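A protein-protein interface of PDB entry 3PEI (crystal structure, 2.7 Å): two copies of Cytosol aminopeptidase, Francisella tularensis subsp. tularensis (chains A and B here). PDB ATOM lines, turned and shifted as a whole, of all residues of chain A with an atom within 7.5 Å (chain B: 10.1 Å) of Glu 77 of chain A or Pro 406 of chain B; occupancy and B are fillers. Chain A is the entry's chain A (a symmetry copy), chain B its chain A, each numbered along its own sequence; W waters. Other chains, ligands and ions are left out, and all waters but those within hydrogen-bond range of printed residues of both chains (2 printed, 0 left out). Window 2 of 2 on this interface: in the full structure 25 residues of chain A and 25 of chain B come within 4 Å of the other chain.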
ATOM      1  N   SER A  49      15.729 -10.324  -3.594  1.00  0.00           N
ATOM      2  CA  SER A  49      14.835 -10.802  -4.640  1.00  0.00           C
ATOM      3  C   SER A  49      14.396 -12.236  -4.391  1.00  0.00           C
ATOM      4  O   SER A  49      15.218 -13.133  -4.399  1.00  0.00           O
ATOM      5  CB  SER A  49      15.507 -10.689  -5.998  1.00  0.00           C
ATOM      6  OG  SER A  49      14.577 -10.869  -7.046  1.00  0.00           O
ATOM      7  N   ASP A  72      18.281  -3.973 -10.057  1.00  0.00           N
ATOM      8  CA  ASP A  72      18.583  -5.377 -10.366  1.00  0.00           C
ATOM      9  C   ASP A  72      17.347  -6.141 -10.816  1.00  0.00           C
ATOM     10  O   ASP A  72      17.389  -7.342 -11.072  1.00  0.00           O
ATOM     11  CB  ASP A  72      19.242  -6.069  -9.175  1.00  0.00           C
ATOM     12  CG  ASP A  72      20.601  -5.486  -8.856  1.00  0.00           C
ATOM     13  OD1 ASP A  72      21.254  -5.004  -9.812  1.00  0.00           O
ATOM     14  OD2 ASP A  72      21.011  -5.489  -7.669  1.00  0.00           O
ATOM     15  N   PHE A  73      16.247  -5.415 -10.930  1.00  0.00           N
ATOM     16  CA  PHE A  73      14.946  -6.023 -11.082  1.00  0.00           C
ATOM     17  C   PHE A  73      14.584  -6.258 -12.540  1.00  0.00           C
ATOM     18  O   PHE A  73      14.478  -5.323 -13.327  1.00  0.00           O
ATOM     19  CB  PHE A  73      13.880  -5.151 -10.412  1.00  0.00           C
ATOM     20  CG  PHE A  73      12.524  -5.783 -10.373  1.00  0.00           C
ATOM     21  CD1 PHE A  73      12.251  -6.803  -9.477  1.00  0.00           C
ATOM     22  CD2 PHE A  73      11.526  -5.371 -11.238  1.00  0.00           C
ATOM     23  CE1 PHE A  73      11.002  -7.393  -9.436  1.00  0.00           C
ATOM     24  CE2 PHE A  73      10.265  -5.963 -11.206  1.00  0.00           C
ATOM     25  CZ  PHE A  73      10.006  -6.972 -10.308  1.00  0.00           C
ATOM     26  N   ILE A  74      14.379  -7.516 -12.892  1.00  0.00           N
ATOM     27  CA  ILE A  74      13.928  -7.822 -14.224  1.00  0.00           C
ATOM     28  C   ILE A  74      12.482  -8.222 -14.109  1.00  0.00           C
ATOM     29  O   ILE A  74      12.157  -9.280 -13.562  1.00  0.00           O
ATOM     30  CB  ILE A  74      14.704  -8.985 -14.815  1.00  0.00           C
ATOM     31  CG1 ILE A  74      16.174  -8.895 -14.399  1.00  0.00           C
ATOM     32  CG2 ILE A  74      14.522  -9.015 -16.324  1.00  0.00           C
ATOM     33  CD1 ILE A  74      16.991  -8.118 -15.325  1.00  0.00           C
ATOM     34  N   ALA A  75      11.615  -7.363 -14.621  1.00  0.00           N
ATOM     35  CA  ALA A  75      10.184  -7.573 -14.528  1.00  0.00           C
ATOM     36  C   ALA A  75       9.725  -8.897 -15.130  1.00  0.00           C
ATOM     37  O   ALA A  75       8.760  -9.494 -14.651  1.00  0.00           O
ATOM     38  CB  ALA A  75       9.446  -6.416 -15.181  1.00  0.00           C
ATOM     39  N   SER A  76      10.384  -9.343 -16.195  1.00  0.00           N
ATOM     40  CA  SER A  76       9.926 -10.548 -16.882  1.00  0.00           C
ATOM     41  C   SER A  76      10.119 -11.787 -15.981  1.00  0.00           C
ATOM     42  O   SER A  76       9.578 -12.861 -16.260  1.00  0.00           O
ATOM     43  CB  SER A  76      10.630 -10.721 -18.238  1.00  0.00           C
ATOM     44  OG  SER A  76      12.037 -10.899 -18.082  1.00  0.00           O
ATOM     45  N   GLU A  77      10.870 -11.608 -14.898  1.00  0.00           N
ATOM     46  CA  GLU A  77      11.154 -12.671 -13.950  1.00  0.00           C
ATOM     47  C   GLU A  77      10.233 -12.636 -12.719  1.00  0.00           C
ATOM     48  O   GLU A  77      10.396 -13.435 -11.795  1.00  0.00           O
ATOM     49  CB  GLU A  77      12.599 -12.548 -13.471  1.00  0.00           C
ATOM     50  CG  GLU A  77      13.634 -12.862 -14.516  1.00  0.00           C
ATOM     51  CD  GLU A  77      13.698 -14.343 -14.839  1.00  0.00           C
ATOM     52  OE1 GLU A  77      14.213 -15.102 -13.983  1.00  0.00           O
ATOM     53  OE2 GLU A  77      13.227 -14.742 -15.936  1.00  0.00           O
ATOM     54  N   TYR A  78       9.286 -11.700 -12.698  1.00  0.00           N
ATOM     55  CA  TYR A  78       8.469 -11.473 -11.519  1.00  0.00           C
ATOM     56  C   TYR A  78       7.635 -12.693 -11.089  1.00  0.00           C
ATOM     57  O   TYR A  78       7.468 -12.933  -9.905  1.00  0.00           O
ATOM     58  CB  TYR A  78       7.604 -10.250 -11.754  1.00  0.00           C
ATOM     59  CG  TYR A  78       6.764  -9.796 -10.590  1.00  0.00           C
ATOM     60  CD1 TYR A  78       7.311  -9.605  -9.328  1.00  0.00           C
ATOM     61  CD2 TYR A  78       5.408  -9.527 -10.764  1.00  0.00           C
ATOM     62  CE1 TYR A  78       6.501  -9.171  -8.248  1.00  0.00           C
ATOM     63  CE2 TYR A  78       4.613  -9.086  -9.720  1.00  0.00           C
ATOM     64  CZ  TYR A  78       5.159  -8.908  -8.466  1.00  0.00           C
ATOM     65  OH  TYR A  78       4.342  -8.479  -7.449  1.00  0.00           O
ATOM     66  N   ASP A  79       7.150 -13.477 -12.044  1.00  0.00           N
ATOM     67  CA  ASP A  79       6.443 -14.723 -11.735  1.00  0.00           C
ATOM     68  C   ASP A  79       7.277 -15.660 -10.887  1.00  0.00           C
ATOM     69  O   ASP A  79       6.746 -16.347 -10.021  1.00  0.00           O
ATOM     70  CB  ASP A  79       6.049 -15.469 -13.009  1.00  0.00           C
ATOM     71  CG  ASP A  79       4.901 -14.805 -13.762  1.00  0.00           C
ATOM     72  OD1 ASP A  79       4.870 -13.559 -13.868  1.00  0.00           O
ATOM     73  OD2 ASP A  79       4.022 -15.539 -14.260  1.00  0.00           O
ATOM     74  N   LYS A  80       8.577 -15.710 -11.152  1.00  0.00           N
ATOM     75  CA  LYS A  80       9.472 -16.583 -10.413  1.00  0.00           C
ATOM     76  C   LYS A  80       9.541 -16.130  -8.964  1.00  0.00           C
ATOM     77  O   LYS A  80       9.683 -16.947  -8.053  1.00  0.00           O
ATOM     78  CB  LYS A  80      10.884 -16.563 -11.009  1.00  0.00           C
ATOM     79  CG  LYS A  80      11.214 -17.647 -12.017  1.00  0.00           C
ATOM     80  CD  LYS A  80      10.813 -17.261 -13.418  1.00  0.00           C
ATOM     81  CE  LYS A  80      11.590 -18.067 -14.466  1.00  0.00           C
ATOM     82  NZ  LYS A  80      13.040 -17.688 -14.532  1.00  0.00           N
ATOM     83  N   ILE A  81       9.445 -14.823  -8.746  1.00  0.00           N
ATOM     84  CA  ILE A  81       9.447 -14.292  -7.382  1.00  0.00           C
ATOM     85  C   ILE A  81       8.118 -14.556  -6.662  1.00  0.00           C
ATOM     86  O   ILE A  81       8.083 -15.043  -5.534  1.00  0.00           O
ATOM     87  CB  ILE A  81       9.717 -12.796  -7.380  1.00  0.00           C
ATOM     88  CG1 ILE A  81      11.132 -12.535  -7.860  1.00  0.00           C
ATOM     89  CG2 ILE A  81       9.531 -12.213  -5.994  1.00  0.00           C
ATOM     90  CD1 ILE A  81      11.418 -11.071  -8.033  1.00  0.00           C
ATOM     91  N   ILE A  82       7.019 -14.207  -7.317  1.00  0.00           N
ATOM     92  CA  ILE A  82       5.717 -14.508  -6.773  1.00  0.00           C
ATOM     93  C   ILE A  82       5.605 -16.008  -6.491  1.00  0.00           C
ATOM     94  O   ILE A  82       5.008 -16.411  -5.501  1.00  0.00           O
ATOM     95  CB  ILE A  82       4.616 -14.023  -7.717  1.00  0.00           C
ATOM     96  CG1 ILE A  82       4.677 -12.506  -7.800  1.00  0.00           C
ATOM     97  CG2 ILE A  82       3.218 -14.476  -7.245  1.00  0.00           C
ATOM     98  CD1 ILE A  82       4.258 -11.852  -6.527  1.00  0.00           C
ATOM     99  N   ALA A  83       6.206 -16.838  -7.333  1.00  0.00           N
ATOM    100  CA  ALA A  83       6.139 -18.280  -7.113  1.00  0.00           C
ATOM    101  C   ALA A  83       6.531 -18.651  -5.677  1.00  0.00           C
ATOM    102  O   ALA A  83       5.904 -19.516  -5.059  1.00  0.00           O
ATOM    103  CB  ALA A  83       7.003 -19.031  -8.140  1.00  0.00           C
ATOM    104  N   ASP A 371      13.725 -20.415 -22.926  1.00  0.00           N
ATOM    105  CA  ASP A 371      12.322 -20.421 -22.502  1.00  0.00           C
ATOM    106  C   ASP A 371      11.768 -19.000 -22.336  1.00  0.00           C
ATOM    107  O   ASP A 371      10.558 -18.815 -22.294  1.00  0.00           O
ATOM    108  CB  ASP A 371      12.174 -21.149 -21.165  1.00  0.00           C
ATOM    109  CG  ASP A 371      12.946 -20.455 -20.035  1.00  0.00           C
ATOM    110  OD1 ASP A 371      12.425 -19.486 -19.407  1.00  0.00           O
ATOM    111  OD2 ASP A 371      14.101 -20.859 -19.783  1.00  0.00           O
ATOM    112  N   ALA A 372      12.656 -18.015 -22.222  1.00  0.00           N
ATOM    113  CA  ALA A 372      12.259 -16.667 -21.839  1.00  0.00           C
ATOM    114  C   ALA A 372      11.568 -15.901 -22.950  1.00  0.00           C
ATOM    115  O   ALA A 372      10.759 -15.025 -22.685  1.00  0.00           O
ATOM    116  CB  ALA A 372      13.456 -15.875 -21.317  1.00  0.00           C
ATOM    117  N   TYR A 373      11.890 -16.213 -24.197  1.00  0.00           N
ATOM    118  CA  TYR A 373      11.323 -15.468 -25.323  1.00  0.00           C
ATOM    119  C   TYR A 373      10.504 -16.372 -26.223  1.00  0.00           C
ATOM    120  O   TYR A 373      10.857 -17.522 -26.453  1.00  0.00           O
ATOM    121  CB  TYR A 373      12.424 -14.798 -26.157  1.00  0.00           C
ATOM    122  CG  TYR A 373      13.259 -13.812 -25.383  1.00  0.00           C
ATOM    123  CD1 TYR A 373      12.937 -12.453 -25.380  1.00  0.00           C
ATOM    124  CD2 TYR A 373      14.375 -14.230 -24.649  1.00  0.00           C
ATOM    125  CE1 TYR A 373      13.695 -11.532 -24.665  1.00  0.00           C
ATOM    126  CE2 TYR A 373      15.138 -13.328 -23.933  1.00  0.00           C
ATOM    127  CZ  TYR A 373      14.791 -11.980 -23.950  1.00  0.00           C
ATOM    128  OH  TYR A 373      15.541 -11.068 -23.255  1.00  0.00           O
ATOM    129  N   ASN A 395       5.441  -7.888 -20.205  1.00  0.00           N
ATOM    130  CA  ASN A 395       6.637  -8.671 -19.884  1.00  0.00           C
ATOM    131  C   ASN A 395       6.517 -10.138 -20.236  1.00  0.00           C
ATOM    132  O   ASN A 395       7.173 -10.974 -19.635  1.00  0.00           O
ATOM    133  CB  ASN A 395       7.051  -8.504 -18.433  1.00  0.00           C
ATOM    134  CG  ASN A 395       7.427  -7.082 -18.122  1.00  0.00           C
ATOM    135  OD1 ASN A 395       8.480  -6.617 -18.547  1.00  0.00           O
ATOM    136  ND2 ASN A 395       6.552  -6.363 -17.412  1.00  0.00           N
ATOM    137  N   LEU A 397       7.816 -11.841 -22.919  1.00  0.00           N
ATOM    138  CA  LEU A 397       8.856 -11.425 -23.852  1.00  0.00           C
ATOM    139  C   LEU A 397       8.860 -12.082 -25.234  1.00  0.00           C
ATOM    140  O   LEU A 397       8.726 -13.303 -25.372  1.00  0.00           O
ATOM    141  CB  LEU A 397      10.197 -11.702 -23.230  1.00  0.00           C
ATOM    142  CG  LEU A 397      10.518 -11.036 -21.922  1.00  0.00           C
ATOM    143  CD1 LEU A 397      12.001 -11.324 -21.610  1.00  0.00           C
ATOM    144  CD2 LEU A 397      10.213  -9.548 -22.018  1.00  0.00           C
ATOM    145  N   PRO B 402      19.378 -11.091 -27.596  1.00  0.00           N
ATOM    146  CA  PRO B 402      19.225 -10.396 -26.310  1.00  0.00           C
ATOM    147  C   PRO B 402      20.223 -10.881 -25.272  1.00  0.00           C
ATOM    148  O   PRO B 402      20.391 -12.094 -25.097  1.00  0.00           O
ATOM    149  CB  PRO B 402      17.799 -10.766 -25.888  1.00  0.00           C
ATOM    150  CG  PRO B 402      17.534 -12.067 -26.561  1.00  0.00           C
ATOM    151  CD  PRO B 402      18.271 -12.023 -27.865  1.00  0.00           C
ATOM    152  N   LEU B 403      20.884  -9.948 -24.597  1.00  0.00           N
ATOM    153  CA  LEU B 403      21.794 -10.311 -23.521  1.00  0.00           C
ATOM    154  C   LEU B 403      20.993 -10.479 -22.228  1.00  0.00           C
ATOM    155  O   LEU B 403      20.976  -9.605 -21.389  1.00  0.00           O
ATOM    156  CB  LEU B 403      22.813  -9.204 -23.376  1.00  0.00           C
ATOM    157  CG  LEU B 403      24.159  -9.488 -22.742  1.00  0.00           C
ATOM    158  CD1 LEU B 403      24.843 -10.628 -23.467  1.00  0.00           C
ATOM    159  CD2 LEU B 403      24.971  -8.202 -22.795  1.00  0.00           C
ATOM    160  N   HIS B 404      20.326 -11.620 -22.082  1.00  0.00           N
ATOM    161  CA  HIS B 404      19.266 -11.809 -21.095  1.00  0.00           C
ATOM    162  C   HIS B 404      19.795 -12.272 -19.732  1.00  0.00           C
ATOM    163  O   HIS B 404      20.024 -13.458 -19.506  1.00  0.00           O
ATOM    164  CB  HIS B 404      18.272 -12.807 -21.681  1.00  0.00           C
ATOM    165  CG  HIS B 404      17.091 -13.088 -20.806  1.00  0.00           C
ATOM    166  ND1 HIS B 404      16.085 -12.172 -20.599  1.00  0.00           N
ATOM    167  CD2 HIS B 404      16.762 -14.188 -20.086  1.00  0.00           C
ATOM    168  CE1 HIS B 404      15.174 -12.702 -19.799  1.00  0.00           C
ATOM    169  NE2 HIS B 404      15.566 -13.918 -19.469  1.00  0.00           N
ATOM    170  N   LYS B 405      19.988 -11.326 -18.821  1.00  0.00           N
ATOM    171  CA  LYS B 405      20.681 -11.621 -17.566  1.00  0.00           C
ATOM    172  C   LYS B 405      20.130 -12.805 -16.759  1.00  0.00           C
ATOM    173  O   LYS B 405      20.888 -13.506 -16.102  1.00  0.00           O
ATOM    174  CB  LYS B 405      20.805 -10.370 -16.685  1.00  0.00           C
ATOM    175  CG  LYS B 405      21.873  -9.408 -17.161  1.00  0.00           C
ATOM    176  CD  LYS B 405      21.862  -8.097 -16.362  1.00  0.00           C
ATOM    177  CE  LYS B 405      22.871  -7.081 -16.953  1.00  0.00           C
ATOM    178  NZ  LYS B 405      22.835  -5.710 -16.323  1.00  0.00           N
ATOM    179  N   PRO B 406      18.814 -13.038 -16.796  1.00  0.00           N
ATOM    180  CA  PRO B 406      18.438 -14.187 -15.961  1.00  0.00           C
ATOM    181  C   PRO B 406      19.094 -15.487 -16.393  1.00  0.00           C
ATOM    182  O   PRO B 406      19.149 -16.397 -15.581  1.00  0.00           O
ATOM    183  CB  PRO B 406      16.927 -14.264 -16.133  1.00  0.00           C
ATOM    184  CG  PRO B 406      16.516 -12.841 -16.397  1.00  0.00           C
ATOM    185  CD  PRO B 406      17.644 -12.251 -17.230  1.00  0.00           C
ATOM    186  N   TYR B 407      19.599 -15.586 -17.621  1.00  0.00           N
ATOM    187  CA  TYR B 407      20.212 -16.841 -18.051  1.00  0.00           C
ATOM    188  C   TYR B 407      21.595 -17.055 -17.425  1.00  0.00           C
ATOM    189  O   TYR B 407      22.163 -18.137 -17.550  1.00  0.00           O
ATOM    190  CB  TYR B 407      20.330 -16.921 -19.564  1.00  0.00           C
ATOM    191  CG  TYR B 407      19.043 -17.178 -20.289  1.00  0.00           C
ATOM    192  CD1 TYR B 407      17.944 -17.721 -19.636  1.00  0.00           C
ATOM    193  CD2 TYR B 407      18.927 -16.878 -21.646  1.00  0.00           C
ATOM    194  CE1 TYR B 407      16.768 -17.944 -20.305  1.00  0.00           C
ATOM    195  CE2 TYR B 407      17.755 -17.107 -22.330  1.00  0.00           C
ATOM    196  CZ  TYR B 407      16.678 -17.639 -21.662  1.00  0.00           C
ATOM    197  OH  TYR B 407      15.516 -17.862 -22.368  1.00  0.00           O
ATOM    198  N   LEU B 408      22.141 -16.024 -16.778  1.00  0.00           N
ATOM    199  CA  LEU B 408      23.275 -16.218 -15.883  1.00  0.00           C
ATOM    200  C   LEU B 408      23.093 -17.420 -14.950  1.00  0.00           C
ATOM    201  O   LEU B 408      24.079 -18.072 -14.595  1.00  0.00           O
ATOM    202  CB  LEU B 408      23.560 -14.964 -15.067  1.00  0.00           C
ATOM    203  CG  LEU B 408      24.801 -14.120 -15.432  1.00  0.00           C
ATOM    204  CD1 LEU B 408      25.596 -14.643 -16.641  1.00  0.00           C
ATOM    205  CD2 LEU B 408      24.487 -12.632 -15.583  1.00  0.00           C
ATOM    206  N   LYS B 409      21.857 -17.739 -14.563  1.00  0.00           N
ATOM    207  CA  LYS B 409      21.641 -18.901 -13.695  1.00  0.00           C
ATOM    208  C   LYS B 409      22.101 -20.201 -14.329  1.00  0.00           C
ATOM    209  O   LYS B 409      22.415 -21.161 -13.632  1.00  0.00           O
ATOM    210  CB  LYS B 409      20.180 -19.048 -13.307  1.00  0.00           C
ATOM    211  CG  LYS B 409      19.748 -18.038 -12.281  1.00  0.00           C
ATOM    212  CD  LYS B 409      18.846 -16.957 -12.896  1.00  0.00           C
ATOM    213  CE  LYS B 409      18.355 -15.987 -11.831  1.00  0.00           C
ATOM    214  NZ  LYS B 409      19.475 -15.176 -11.249  1.00  0.00           N
ATOM    215  N   LYS B 410      22.123 -20.245 -15.654  1.00  0.00           N
ATOM    216  CA  LYS B 410      22.473 -21.471 -16.340  1.00  0.00           C
ATOM    217  C   LYS B 410      23.962 -21.788 -16.170  1.00  0.00           C
ATOM    218  O   LYS B 410      24.421 -22.876 -16.511  1.00  0.00           O
ATOM    219  CB  LYS B 410      22.112 -21.376 -17.815  1.00  0.00           C
ATOM    220  CG  LYS B 410      20.643 -21.364 -18.085  1.00  0.00           C
ATOM    221  CD  LYS B 410      20.385 -21.098 -19.567  1.00  0.00           C
ATOM    222  CE  LYS B 410      18.969 -21.424 -19.959  1.00  0.00           C
ATOM    223  NZ  LYS B 410      18.647 -22.790 -19.427  1.00  0.00           N
ATOM    224  N   ILE B 411      24.736 -20.840 -15.661  1.00  0.00           N
ATOM    225  CA  ILE B 411      26.152 -21.108 -15.435  1.00  0.00           C
ATOM    226  C   ILE B 411      26.549 -20.818 -14.002  1.00  0.00           C
ATOM    227  O   ILE B 411      27.661 -20.400 -13.711  1.00  0.00           O
ATOM    228  CB  ILE B 411      27.078 -20.355 -16.412  1.00  0.00           C
ATOM    229  CG1 ILE B 411      26.741 -18.860 -16.438  1.00  0.00           C
ATOM    230  CG2 ILE B 411      26.998 -20.984 -17.789  1.00  0.00           C
ATOM    231  CD1 ILE B 411      27.412 -18.090 -17.569  1.00  0.00           C
ATOM    232  N   GLU B 412      25.612 -21.019 -13.100  1.00  0.00           N
ATOM    233  CA  GLU B 412      25.961 -21.038 -11.708  1.00  0.00           C
ATOM    234  C   GLU B 412      26.731 -22.317 -11.493  1.00  0.00           C
ATOM    235  O   GLU B 412      26.596 -23.285 -12.249  1.00  0.00           O
ATOM    236  CB  GLU B 412      24.737 -20.929 -10.822  1.00  0.00           C
ATOM    237  CG  GLU B 412      24.500 -19.479 -10.410  1.00  0.00           C
ATOM    238  CD  GLU B 412      23.083 -19.217  -9.932  1.00  0.00           C
ATOM    239  OE1 GLU B 412      22.582 -18.091 -10.186  1.00  0.00           O
ATOM    240  OE2 GLU B 412      22.475 -20.134  -9.315  1.00  0.00           O
ATOM    241  N   SER B 426      20.479 -25.128 -24.631  1.00  0.00           N
ATOM    242  CA  SER B 426      19.501 -24.045 -24.724  1.00  0.00           C
ATOM    243  C   SER B 426      20.057 -22.635 -24.465  1.00  0.00           C
ATOM    244  O   SER B 426      20.756 -22.390 -23.473  1.00  0.00           O
ATOM    245  CB  SER B 426      18.288 -24.307 -23.835  1.00  0.00           C
ATOM    246  OG  SER B 426      18.670 -24.249 -22.491  1.00  0.00           O
ATOM    247  N   ALA B 427      19.714 -21.719 -25.373  1.00  0.00           N
ATOM    248  CA  ALA B 427      20.186 -20.349 -25.329  1.00  0.00           C
ATOM    249  C   ALA B 427      21.711 -20.322 -25.251  1.00  0.00           C
ATOM    250  O   ALA B 427      22.315 -19.392 -24.708  1.00  0.00           O
ATOM    251  CB  ALA B 427      19.558 -19.608 -24.169  1.00  0.00           C
ATOM    252  N   ILE B 430      23.592 -17.193 -26.242  1.00  0.00           N
ATOM    253  CA  ILE B 430      23.273 -16.156 -25.271  1.00  0.00           C
ATOM    254  C   ILE B 430      24.065 -16.396 -23.996  1.00  0.00           C
ATOM    255  O   ILE B 430      24.670 -15.469 -23.430  1.00  0.00           O
ATOM    256  CB  ILE B 430      21.775 -16.118 -24.973  1.00  0.00           C
ATOM    257  CG1 ILE B 430      21.011 -15.725 -26.239  1.00  0.00           C
ATOM    258  CG2 ILE B 430      21.468 -15.181 -23.803  1.00  0.00           C
ATOM    259  CD1 ILE B 430      19.528 -15.805 -26.080  1.00  0.00           C
ATOM    260  N   VAL B 431      24.105 -17.656 -23.578  1.00  0.00           N
ATOM    261  CA  VAL B 431      24.881 -18.027 -22.402  1.00  0.00           C
ATOM    262  C   VAL B 431      26.371 -17.675 -22.579  1.00  0.00           C
ATOM    263  O   VAL B 431      27.013 -17.115 -21.684  1.00  0.00           O
ATOM    264  CB  VAL B 431      24.701 -19.524 -22.054  1.00  0.00           C
ATOM    265  CG1 VAL B 431      25.744 -19.958 -21.074  1.00  0.00           C
ATOM    266  CG2 VAL B 431      23.321 -19.777 -21.467  1.00  0.00           C
ATOM    267  N   LEU B 434      26.802 -14.037 -22.257  1.00  0.00           N
ATOM    268  CA  LEU B 434      26.648 -13.666 -20.846  1.00  0.00           C
ATOM    269  C   LEU B 434      27.913 -13.958 -20.033  1.00  0.00           C
ATOM    270  O   LEU B 434      28.349 -13.137 -19.224  1.00  0.00           O
ATOM    271  CB  LEU B 434      25.445 -14.373 -20.195  1.00  0.00           C
ATOM    272  CG  LEU B 434      24.095 -13.783 -20.617  1.00  0.00           C
ATOM    273  CD1 LEU B 434      22.917 -14.666 -20.241  1.00  0.00           C
ATOM    274  CD2 LEU B 434      23.920 -12.370 -20.092  1.00  0.00           C
ATOM    275  N   SER B 437      30.199 -11.301 -20.799  1.00  0.00           N
ATOM    276  CA  SER B 437      29.715 -10.015 -20.341  1.00  0.00           C
ATOM    277  C   SER B 437      30.097  -9.761 -18.901  1.00  0.00           C
ATOM    278  O   SER B 437      30.100  -8.625 -18.467  1.00  0.00           O
ATOM    279  CB  SER B 437      28.203  -9.918 -20.488  1.00  0.00           C
ATOM    280  OG  SER B 437      27.566 -10.631 -19.447  1.00  0.00           O
ATOM    281  N   LYS B 438      30.406 -10.817 -18.159  1.00  0.00           N
ATOM    282  CA  LYS B 438      30.903 -10.655 -16.789  1.00  0.00           C
ATOM    283  C   LYS B 438      32.269  -9.980 -16.776  1.00  0.00           C
ATOM    284  O   LYS B 438      32.696  -9.489 -15.747  1.00  0.00           O
ATOM    285  CB  LYS B 438      31.021 -11.997 -16.052  1.00  0.00           C
ATOM    286  CG  LYS B 438      29.726 -12.701 -15.776  1.00  0.00           C
ATOM    287  CD  LYS B 438      28.657 -11.738 -15.263  1.00  0.00           C
ATOM    288  CE  LYS B 438      28.717 -11.543 -13.745  1.00  0.00           C
ATOM    289  NZ  LYS B 438      27.695 -10.526 -13.302  1.00  0.00           N
HETATM  290  O   HOH W   1      12.562 -13.541 -17.937  1.00  0.00           O
HETATM  291  O   HOH W   2      14.181 -16.288 -18.084  1.00  0.00           O
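A ring nitrogen (ND1) of His 404 of chain B lies within hydrogen-bond range of the side-chain hydroxyl (OH) of Tyr 373 of chain A.
The backbone NH (N) of Asp 371 of chain A is in hydrogen-bond range of the side-chain hydroxyl (OH) of Tyr 407 of chain B (3.2 Å).
The side-chain hydroxyl of Tyr 407 of chain B lies within hydrogen-bond range of the backbone NH of Ala 372 of chain A, at 2.9 Å.
Water W1 lies within hydrogen-bond range of the side-chain carboxylate (OE2) of Glu 77 of chain A (2.4 Å), the side-chain hydroxyl (OG) of Ser 76 of chain A (2.7 Å) and a ring nitrogen (NE2) of His 404 of chain B (3.4 Å).
Water W2 bridges the side-chain carboxylate of Glu 77 of chain A and a ring nitrogen (NE2) of His 404 of chain B.
Among the printed residues, merely in contact across the chains: Glu 77 of chain A with Pro 406 of chain B (3.4 Å), Ala 372 of chain A with His 404 of chain B (3.4 Å), Tyr 373 of chain A with Pro 402 of chain B (3.5 Å) and Leu 397 of chain A with His 404 of chain B (3.9 Å).
No residue of chain B comes within 4 Å of Ile 74 of chain A.
No residue of chain B comes within 4 Å of Ala 75 of chain A.
Of chain B, only Pro 406 comes within 4 Å of Glu 77 of chain A.
Asp 79 of chain A touches none of the printed residues of chain B.
Lys 80 of chain A touches none of the printed residues of chain B.
Printed residues of chain B within 4 Å of Tyr 373 of chain A: Pro 402 and His 404.
Of the printed residues of chain B, Leu 397 of chain A touches His 404.
Of the printed residues of chain A, Pro 402 of chain B touches Tyr 373 (3.5 Å).
Of chain A, only Glu 77 (3.4 Å) comes within 4 Å of Pro 406 of chain B.
Printed residues of chain A within 4 Å of Tyr 407 of chain B: Asp 371 and Ala 372.
Ser 437 of chain B touches none of the printed residues of chain A.
Of the 18 printed residues of chain A, 5 touch a printed residue of chain B.
Printed residues of chain A that touch a printed residue of chain B: Glu 77, Asp 371, Ala 372, Tyr 373 and Leu 397.
Printed residues of chain B that touch a printed residue of chain A: Pro 402, His 404, Pro 406 and Tyr 407.
Among the printed residues, no Asp or Glu carboxylate lies within 4 Å of a Lys or Arg side-chain nitrogen of the other chain.
No position is printed for both chains.
Of the 7 pairs that touch across the chains among the printed residues, none has its exchanged pair printed and touching as well.
OE1 of Glu 77 of chain A is in salt-bridge range of NZ of Lys 80 of chain A (2.9 Å).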
